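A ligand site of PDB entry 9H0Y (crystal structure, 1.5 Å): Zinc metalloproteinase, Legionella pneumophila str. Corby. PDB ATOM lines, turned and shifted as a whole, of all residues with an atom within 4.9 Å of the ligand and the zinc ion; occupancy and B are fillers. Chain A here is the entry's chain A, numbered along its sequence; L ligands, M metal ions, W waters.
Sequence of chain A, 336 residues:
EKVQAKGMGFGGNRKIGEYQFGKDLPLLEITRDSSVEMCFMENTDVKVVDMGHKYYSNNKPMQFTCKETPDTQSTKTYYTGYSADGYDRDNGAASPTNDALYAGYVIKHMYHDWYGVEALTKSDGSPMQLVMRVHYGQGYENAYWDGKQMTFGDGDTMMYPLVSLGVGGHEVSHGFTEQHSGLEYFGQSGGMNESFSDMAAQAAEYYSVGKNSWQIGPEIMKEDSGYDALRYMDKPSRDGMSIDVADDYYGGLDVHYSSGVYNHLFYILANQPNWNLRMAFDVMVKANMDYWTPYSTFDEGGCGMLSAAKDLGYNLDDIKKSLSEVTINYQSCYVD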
ATOM      1  N   GLU A 141      -5.687 -22.330 -16.207  1.00  0.00           N
ATOM      2  CA  GLU A 141      -5.690 -21.709 -14.881  1.00  0.00           C
ATOM      3  C   GLU A 141      -6.632 -22.470 -13.955  1.00  0.00           C
ATOM      4  O   GLU A 141      -7.614 -21.926 -13.419  1.00  0.00           O
ATOM      5  CB  GLU A 141      -6.060 -20.237 -14.987  1.00  0.00           C
ATOM      6  CG  GLU A 141      -5.149 -19.439 -15.927  1.00  0.00           C
ATOM      7  CD  GLU A 141      -5.159 -17.931 -15.688  1.00  0.00           C
ATOM      8  OE1 GLU A 141      -6.187 -17.329 -16.009  1.00  0.00           O
ATOM      9  OE2 GLU A 141      -4.108 -17.335 -15.321  1.00  0.00           O
ATOM     10  N   ASN A 142      -6.327 -23.747 -13.787  1.00  0.00           N
ATOM     11  CA  ASN A 142      -7.085 -24.601 -12.886  1.00  0.00           C
ATOM     12  C   ASN A 142      -6.295 -25.881 -12.611  1.00  0.00           C
ATOM     13  O   ASN A 142      -5.197 -26.096 -13.135  1.00  0.00           O
ATOM     14  CB  ASN A 142      -8.457 -24.954 -13.469  1.00  0.00           C
ATOM     15  CG  ASN A 142      -9.560 -24.867 -12.433  1.00  0.00           C
ATOM     16  OD1 ASN A 142      -9.345 -25.128 -11.246  1.00  0.00           O
ATOM     17  ND2 ASN A 142     -10.772 -24.569 -12.890  1.00  0.00           N
ATOM     18  N   ALA A 143      -6.895 -26.734 -11.782  1.00  0.00           N
ATOM     19  CA  ALA A 143      -6.432 -28.085 -11.469  1.00  0.00           C
ATOM     20  C   ALA A 143      -7.696 -28.929 -11.308  1.00  0.00           C
ATOM     21  O   ALA A 143      -8.789 -28.384 -11.115  1.00  0.00           O
ATOM     22  CB  ALA A 143      -5.554 -28.107 -10.210  1.00  0.00           C
ATOM     23  N   TYR A 144      -7.548 -30.253 -11.390  1.00  0.00           N
ATOM     24  CA  TYR A 144      -8.742 -31.085 -11.265  1.00  0.00           C
ATOM     25  C   TYR A 144      -8.380 -32.515 -10.878  1.00  0.00           C
ATOM     26  O   TYR A 144      -7.272 -33.004 -11.161  1.00  0.00           O
ATOM     27  CB  TYR A 144      -9.587 -31.070 -12.557  1.00  0.00           C
ATOM     28  CG  TYR A 144      -8.973 -31.789 -13.762  1.00  0.00           C
ATOM     29  CD1 TYR A 144      -8.185 -31.108 -14.678  1.00  0.00           C
ATOM     30  CD2 TYR A 144      -9.263 -33.127 -14.000  1.00  0.00           C
ATOM     31  CE1 TYR A 144      -7.628 -31.780 -15.764  1.00  0.00           C
ATOM     32  CE2 TYR A 144      -8.733 -33.785 -15.090  1.00  0.00           C
ATOM     33  CZ  TYR A 144      -7.918 -33.111 -15.965  1.00  0.00           C
ATOM     34  OH  TYR A 144      -7.404 -33.802 -17.035  1.00  0.00           O
ATOM     35  N   MET A 159      -2.608 -16.501 -12.798  1.00  0.00           N
ATOM     36  CA  MET A 159      -2.110 -17.477 -11.850  1.00  0.00           C
ATOM     37  C   MET A 159      -0.785 -18.042 -12.321  1.00  0.00           C
ATOM     38  O   MET A 159      -0.578 -18.240 -13.521  1.00  0.00           O
ATOM     39  CB  MET A 159      -3.096 -18.638 -11.696  1.00  0.00           C
ATOM     40  CG  MET A 159      -4.434 -18.215 -11.190  1.00  0.00           C
ATOM     41  SD  MET A 159      -5.593 -19.576 -11.137  1.00  0.00           S
ATOM     42  CE  MET A 159      -7.097 -18.642 -11.238  1.00  0.00           C
ATOM     43  N   LEU A 162      -0.254 -24.066 -10.939  1.00  0.00           N
ATOM     44  CA  LEU A 162      -1.096 -24.367  -9.790  1.00  0.00           C
ATOM     45  C   LEU A 162      -0.627 -25.652  -9.103  1.00  0.00           C
ATOM     46  O   LEU A 162      -1.361 -26.632  -8.953  1.00  0.00           O
ATOM     47  CB  LEU A 162      -2.554 -24.470 -10.225  1.00  0.00           C
ATOM     48  CG  LEU A 162      -3.259 -23.193 -10.665  1.00  0.00           C
ATOM     49  CD1 LEU A 162      -3.071 -22.962 -12.157  1.00  0.00           C
ATOM     50  CD2 LEU A 162      -4.738 -23.287 -10.309  1.00  0.00           C
ATOM     51  N   VAL A 167      -2.912 -26.630  -3.171  1.00  0.00           N
ATOM     52  CA  VAL A 167      -3.663 -27.052  -4.346  1.00  0.00           C
ATOM     53  C   VAL A 167      -3.581 -28.570  -4.490  1.00  0.00           C
ATOM     54  O   VAL A 167      -4.583 -29.230  -4.767  1.00  0.00           O
ATOM     55  CB  VAL A 167      -3.169 -26.335  -5.618  1.00  0.00           C
ATOM     56  CG1 VAL A 167      -3.857 -26.938  -6.841  1.00  0.00           C
ATOM     57  CG2 VAL A 167      -3.446 -24.837  -5.520  1.00  0.00           C
ATOM     58  N   HIS A 170      -5.846 -30.176  -1.881  1.00  0.00           N
ATOM     59  CA  HIS A 170      -7.232 -30.041  -2.299  1.00  0.00           C
ATOM     60  C   HIS A 170      -7.596 -31.098  -3.328  1.00  0.00           C
ATOM     61  O   HIS A 170      -8.617 -31.794  -3.196  1.00  0.00           O
ATOM     62  CB  HIS A 170      -7.432 -28.639  -2.844  1.00  0.00           C
ATOM     63  CG  HIS A 170      -8.814 -28.317  -3.273  1.00  0.00           C
ATOM     64  ND1 HIS A 170      -9.660 -27.480  -2.566  1.00  0.00           N
ATOM     65  CD2 HIS A 170      -9.530 -28.792  -4.311  1.00  0.00           C
ATOM     66  CE1 HIS A 170     -10.804 -27.405  -3.201  1.00  0.00           C
ATOM     67  NE2 HIS A 170     -10.757 -28.192  -4.252  1.00  0.00           N
ATOM     68  N   GLU A 171      -6.759 -31.276  -4.355  1.00  0.00           N
ATOM     69  CA  GLU A 171      -7.117 -32.195  -5.430  1.00  0.00           C
ATOM     70  C   GLU A 171      -7.037 -33.649  -4.977  1.00  0.00           C
ATOM     71  O   GLU A 171      -7.944 -34.438  -5.264  1.00  0.00           O
ATOM     72  CB  GLU A 171      -6.237 -31.952  -6.658  1.00  0.00           C
ATOM     73  CG  GLU A 171      -6.436 -30.585  -7.314  1.00  0.00           C
ATOM     74  CD  GLU A 171      -7.867 -30.309  -7.758  1.00  0.00           C
ATOM     75  OE1 GLU A 171      -8.687 -31.252  -7.822  1.00  0.00           O
ATOM     76  OE2 GLU A 171      -8.165 -29.134  -8.036  1.00  0.00           O
ATOM     77  N   HIS A 174     -10.131 -34.562  -3.045  1.00  0.00           N
ATOM     78  CA  HIS A 174     -11.354 -34.903  -3.786  1.00  0.00           C
ATOM     79  C   HIS A 174     -11.435 -36.413  -3.959  1.00  0.00           C
ATOM     80  O   HIS A 174     -12.509 -37.024  -3.867  1.00  0.00           O
ATOM     81  CB  HIS A 174     -11.361 -34.209  -5.139  1.00  0.00           C
ATOM     82  CG  HIS A 174     -11.947 -32.849  -5.120  1.00  0.00           C
ATOM     83  ND1 HIS A 174     -13.146 -32.532  -4.496  1.00  0.00           N
ATOM     84  CD2 HIS A 174     -11.479 -31.701  -5.648  1.00  0.00           C
ATOM     85  CE1 HIS A 174     -13.398 -31.253  -4.660  1.00  0.00           C
ATOM     86  NE2 HIS A 174     -12.401 -30.725  -5.354  1.00  0.00           N
ATOM     87  N   TYR A 185     -21.286 -34.058  -5.935  1.00  0.00           N
ATOM     88  CA  TYR A 185     -20.673 -32.765  -6.264  1.00  0.00           C
ATOM     89  C   TYR A 185     -21.681 -31.744  -6.787  1.00  0.00           C
ATOM     90  O   TYR A 185     -21.522 -31.178  -7.876  1.00  0.00           O
ATOM     91  CB  TYR A 185     -19.547 -32.966  -7.260  1.00  0.00           C
ATOM     92  CG  TYR A 185     -18.506 -31.884  -7.261  1.00  0.00           C
ATOM     93  CD1 TYR A 185     -17.749 -31.615  -6.141  1.00  0.00           C
ATOM     94  CD2 TYR A 185     -18.259 -31.149  -8.421  1.00  0.00           C
ATOM     95  CE1 TYR A 185     -16.770 -30.628  -6.151  1.00  0.00           C
ATOM     96  CE2 TYR A 185     -17.298 -30.164  -8.444  1.00  0.00           C
ATOM     97  CZ  TYR A 185     -16.558 -29.906  -7.314  1.00  0.00           C
ATOM     98  OH  TYR A 185     -15.592 -28.923  -7.351  1.00  0.00           O
ATOM     99  N   GLU A 194     -16.273 -29.693  -1.540  1.00  0.00           N
ATOM    100  CA  GLU A 194     -15.313 -28.619  -1.766  1.00  0.00           C
ATOM    101  C   GLU A 194     -14.631 -28.205  -0.472  1.00  0.00           C
ATOM    102  O   GLU A 194     -13.409 -28.021  -0.437  1.00  0.00           O
ATOM    103  CB  GLU A 194     -16.053 -27.433  -2.378  1.00  0.00           C
ATOM    104  CG  GLU A 194     -15.956 -27.319  -3.872  1.00  0.00           C
ATOM    105  CD  GLU A 194     -14.545 -27.476  -4.377  1.00  0.00           C
ATOM    106  OE1 GLU A 194     -13.743 -26.568  -4.084  1.00  0.00           O
ATOM    107  OE2 GLU A 194     -14.260 -28.453  -5.104  1.00  0.00           O
ATOM    108  N   SER A 197     -11.890 -30.497   0.846  1.00  0.00           N
ATOM    109  CA  SER A 197     -10.663 -30.332   0.071  1.00  0.00           C
ATOM    110  C   SER A 197      -9.940 -29.045   0.461  1.00  0.00           C
ATOM    111  O   SER A 197      -8.692 -29.034   0.495  1.00  0.00           O
ATOM    112  CB  SER A 197     -10.996 -30.381  -1.431  1.00  0.00           C
ATOM    113  OG  SER A 197     -11.134 -31.714  -1.893  1.00  0.00           O
ATOM    114  N   ILE A 216      -6.968 -20.118   0.267  1.00  0.00           N
ATOM    115  CA  ILE A 216      -6.743 -21.076  -0.813  1.00  0.00           C
ATOM    116  C   ILE A 216      -6.119 -20.325  -1.974  1.00  0.00           C
ATOM    117  O   ILE A 216      -6.696 -19.352  -2.482  1.00  0.00           O
ATOM    118  CB  ILE A 216      -8.038 -21.782  -1.238  1.00  0.00           C
ATOM    119  CG1 ILE A 216      -8.680 -22.493  -0.034  1.00  0.00           C
ATOM    120  CG2 ILE A 216      -7.747 -22.762  -2.361  1.00  0.00           C
ATOM    121  CD1 ILE A 216      -7.897 -23.652   0.538  1.00  0.00           C
ATOM    122  N   LEU A 230      -7.734 -17.266  -3.978  1.00  0.00           N
ATOM    123  CA  LEU A 230      -8.969 -17.832  -4.535  1.00  0.00           C
ATOM    124  C   LEU A 230     -10.105 -17.774  -3.516  1.00  0.00           C
ATOM    125  O   LEU A 230     -11.227 -17.360  -3.851  1.00  0.00           O
ATOM    126  CB  LEU A 230      -8.741 -19.286  -4.970  1.00  0.00           C
ATOM    127  CG  LEU A 230      -7.729 -19.546  -6.079  1.00  0.00           C
ATOM    128  CD1 LEU A 230      -7.524 -21.026  -6.324  1.00  0.00           C
ATOM    129  CD2 LEU A 230      -8.194 -18.864  -7.355  1.00  0.00           C
ATOM    130  N   ARG A 231      -9.848 -18.198  -2.280  1.00  0.00           N
ATOM    131  CA  ARG A 231     -10.874 -18.253  -1.245  1.00  0.00           C
ATOM    132  C   ARG A 231     -10.230 -17.917   0.101  1.00  0.00           C
ATOM    133  O   ARG A 231      -9.028 -18.108   0.306  1.00  0.00           O
ATOM    134  CB  ARG A 231     -11.519 -19.637  -1.148  1.00  0.00           C
ATOM    135  CG  ARG A 231     -12.487 -19.952  -2.258  1.00  0.00           C
ATOM    136  CD  ARG A 231     -13.043 -21.378  -2.164  1.00  0.00           C
ATOM    137  NE  ARG A 231     -12.032 -22.389  -2.484  1.00  0.00           N
ATOM    138  CZ  ARG A 231     -11.819 -22.871  -3.699  1.00  0.00           C
ATOM    139  NH1 ARG A 231     -12.264 -22.247  -4.776  1.00  0.00           N
ATOM    140  NH2 ARG A 231     -11.120 -23.994  -3.844  1.00  0.00           N
ATOM    141  N   ASP A 254     -23.047 -22.221  -6.535  1.00  0.00           N
ATOM    142  CA  ASP A 254     -22.071 -23.237  -6.912  1.00  0.00           C
ATOM    143  C   ASP A 254     -21.320 -23.759  -5.687  1.00  0.00           C
ATOM    144  O   ASP A 254     -21.174 -23.059  -4.681  1.00  0.00           O
ATOM    145  CB  ASP A 254     -21.066 -22.656  -7.916  1.00  0.00           C
ATOM    146  CG  ASP A 254     -20.087 -23.678  -8.419  1.00  0.00           C
ATOM    147  OD1 ASP A 254     -20.506 -24.514  -9.251  1.00  0.00           O
ATOM    148  OD2 ASP A 254     -18.918 -23.662  -7.970  1.00  0.00           O
ATOM    149  N   HIS A 256     -18.288 -24.062  -5.125  1.00  0.00           N
ATOM    150  CA  HIS A 256     -17.103 -23.272  -4.790  1.00  0.00           C
ATOM    151  C   HIS A 256     -17.433 -22.024  -3.978  1.00  0.00           C
ATOM    152  O   HIS A 256     -16.509 -21.335  -3.535  1.00  0.00           O
ATOM    153  CB  HIS A 256     -16.374 -22.891  -6.083  1.00  0.00           C
ATOM    154  CG  HIS A 256     -15.786 -24.076  -6.784  1.00  0.00           C
ATOM    155  ND1 HIS A 256     -16.420 -24.708  -7.819  1.00  0.00           N
ATOM    156  CD2 HIS A 256     -14.615 -24.738  -6.587  1.00  0.00           C
ATOM    157  CE1 HIS A 256     -15.685 -25.734  -8.229  1.00  0.00           C
ATOM    158  NE2 HIS A 256     -14.588 -25.763  -7.501  1.00  0.00           N
ATOM    159  N   TYR A 257     -18.713 -21.734  -3.796  1.00  0.00           N
ATOM    160  CA  TYR A 257     -19.200 -20.632  -2.978  1.00  0.00           C
ATOM    161  C   TYR A 257     -19.935 -21.126  -1.740  1.00  0.00           C
ATOM    162  O   TYR A 257     -19.781 -20.559  -0.662  1.00  0.00           O
ATOM    163  CB  TYR A 257     -20.118 -19.750  -3.829  1.00  0.00           C
ATOM    164  CG  TYR A 257     -19.421 -19.197  -5.077  1.00  0.00           C
ATOM    165  CD1 TYR A 257     -18.131 -18.695  -5.024  1.00  0.00           C
ATOM    166  CD2 TYR A 257     -20.066 -19.214  -6.310  1.00  0.00           C
ATOM    167  CE1 TYR A 257     -17.501 -18.207  -6.164  1.00  0.00           C
ATOM    168  CE2 TYR A 257     -19.444 -18.724  -7.453  1.00  0.00           C
ATOM    169  CZ  TYR A 257     -18.164 -18.220  -7.373  1.00  0.00           C
ATOM    170  OH  TYR A 257     -17.521 -17.736  -8.493  1.00  0.00           O
HETATM  171  C1  LIG L   1     -15.591 -21.195  -9.088  1.00  0.00           C
HETATM  172  C2  LIG L   1     -16.913 -20.946  -9.401  1.00  0.00           C
HETATM  173  C3  LIG L   1     -17.584 -21.775 -10.286  1.00  0.00           C
HETATM  174  C4  LIG L   1     -16.936 -22.859 -10.851  1.00  0.00           C
HETATM  175  C5  LIG L   1     -15.613 -23.108 -10.539  1.00  0.00           C
HETATM  176  C6  LIG L   1     -14.939 -22.273  -9.660  1.00  0.00           C
HETATM  177  C7  LIG L   1     -10.957 -20.392 -10.119  1.00  0.00           C
HETATM  178  C8  LIG L   1      -8.965 -21.901 -10.074  1.00  0.00           C
HETATM  179  C9  LIG L   1     -10.827 -24.603  -7.794  1.00  0.00           C
HETATM  180  C10 LIG L   1     -10.296 -26.021  -7.994  1.00  0.00           C
HETATM  181  C11 LIG L   1      -9.374 -26.212  -6.783  1.00  0.00           C
HETATM  182  C12 LIG L   1      -8.303 -25.147  -6.584  1.00  0.00           C
HETATM  183  C13 LIG L   1      -7.332 -25.107  -7.744  1.00  0.00           C
HETATM  184  C14 LIG L   1      -7.567 -25.434  -5.260  1.00  0.00           C
HETATM  185  C15 LIG L   1     -12.544 -22.251  -8.860  1.00  0.00           C
HETATM  186  C16 LIG L   1     -11.260 -22.850  -9.449  1.00  0.00           C
HETATM  187  C17 LIG L   1     -10.478 -21.834 -10.314  1.00  0.00           C
HETATM  188  N1  LIG L   1     -13.600 -22.704  -9.533  1.00  0.00           N
HETATM  189  N2  LIG L   1     -10.392 -23.711  -8.685  1.00  0.00           N
HETATM  190  O1  LIG L   1     -12.530 -21.367  -7.998  1.00  0.00           O
HETATM  191  O2  LIG L   1     -12.156 -27.134  -9.528  1.00  0.00           O
HETATM  192  O3  LIG L   1     -10.565 -28.711  -8.342  1.00  0.00           O
HETATM  193  O4  LIG L   1     -12.380 -27.471  -7.078  1.00  0.00           O
HETATM  194  O5  LIG L   1     -11.509 -24.301  -6.810  1.00  0.00           O
HETATM  195  P1  LIG L   1     -11.406 -27.425  -8.214  1.00  0.00           P
HETATM  196 CL1  LIG L   1     -19.231 -21.406 -10.708  1.00  0.00          CL
HETATM  197 CL2  LIG L   1     -17.771 -23.952 -11.897  1.00  0.00          CL
HETATM  198 ZN    ZN M   1     -12.339 -28.640  -5.559  1.00  0.00          ZN
HETATM  199  O   HOH W   1     -11.474 -31.172  -9.463  1.00  0.00           O
HETATM  200  O   HOH W   2     -12.929 -25.114 -11.159  1.00  0.00           O
HETATM  201  O   HOH W   3     -14.703 -28.440  -9.820  1.00  0.00           O
HETATM  202  O   HOH W   4     -11.469 -28.321 -11.715  1.00  0.00           O
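The side-chain carboxylate (OE2) of Glu 171 sits close to an oxygen (O3) of the ligand, at 2.5 Å. O5 of the ligand sits at hydrogen-bond distance from NH1 of Arg 231, 3.0 Å away. A ring nitrogen (NE2) of His 256 lies within hydrogen-bond range of an oxygen (O2) of the ligand, at 3.5 Å. The side-chain amide oxygen of Asn 142 lies within hydrogen-bond range of a nitrogen (N2) of the ligand, at 3.1 Å.
OE2 of Glu 141 lies within hydrogen-bond range of N of Met 159. O of Ile 216 sits at hydrogen-bond distance from N of Leu 230 (2.8 Å). OE1 of Glu 194 is in salt-bridge range of NH2 of Arg 231 (3.7 Å). The side-chain hydroxyl of Tyr 185 lies close to the side-chain carboxylate of Glu 194 (2.7 Å). A ring nitrogen (ND1) of His 256 sits at hydrogen-bond distance from the side-chain carboxylate (OD2) of Asp 254. The backbone carbonyl oxygen (O) of His 170 is in hydrogen-bond range of the side-chain hydroxyl (OG) of Ser 197, 2.8 Å away. The backbone carbonyl oxygen (O) of Arg 231 lies within hydrogen-bond range of the backbone NH (N) of Ile 216, 2.9 Å away. NE2 of His 256 lies close to OH of Tyr 185 (3.3 Å).
O of Ala 143 lies close to O3 of the ligand, at 3.3 Å. Merely in contact with the ligand: Asp 254, Tyr 257, Tyr 185, Glu 141, Met 159 and Ile 216.
Residues that only touch the zinc ion: Tyr 185 (3.7 Å). Within 4 Å of the zinc ion: His 170, His 174, Tyr 185 and Glu 194.
An oxygen (O4) of the ligand is bound to the zinc ion (1.9 Å). The zinc ion is bound by OE2 of Glu 194. A ring nitrogen (NE2) of His 174 is bound to the zinc ion (2.1 Å). The zinc ion is bound by NE2 of His 170, at 2.1 Å. The zinc ion has four donor atoms within binding distance.
Water W4 bridges an oxygen (O2) of the ligand (2.6 Å) and the backbone carbonyl oxygen (O) of Ala 143 (2.7 Å). Water W2 bridges an oxygen (O2) of the ligand and the side-chain amide nitrogen (ND2) of Asn 142. Water W1 bridges an oxygen (O3) of the ligand (2.9 Å) and the side-chain carboxylate (OE1) of Glu 171 (3.2 Å). Water W3 bridges OH of Tyr 185 (2.7 Å) and O2 of the ligand (2.9 Å).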
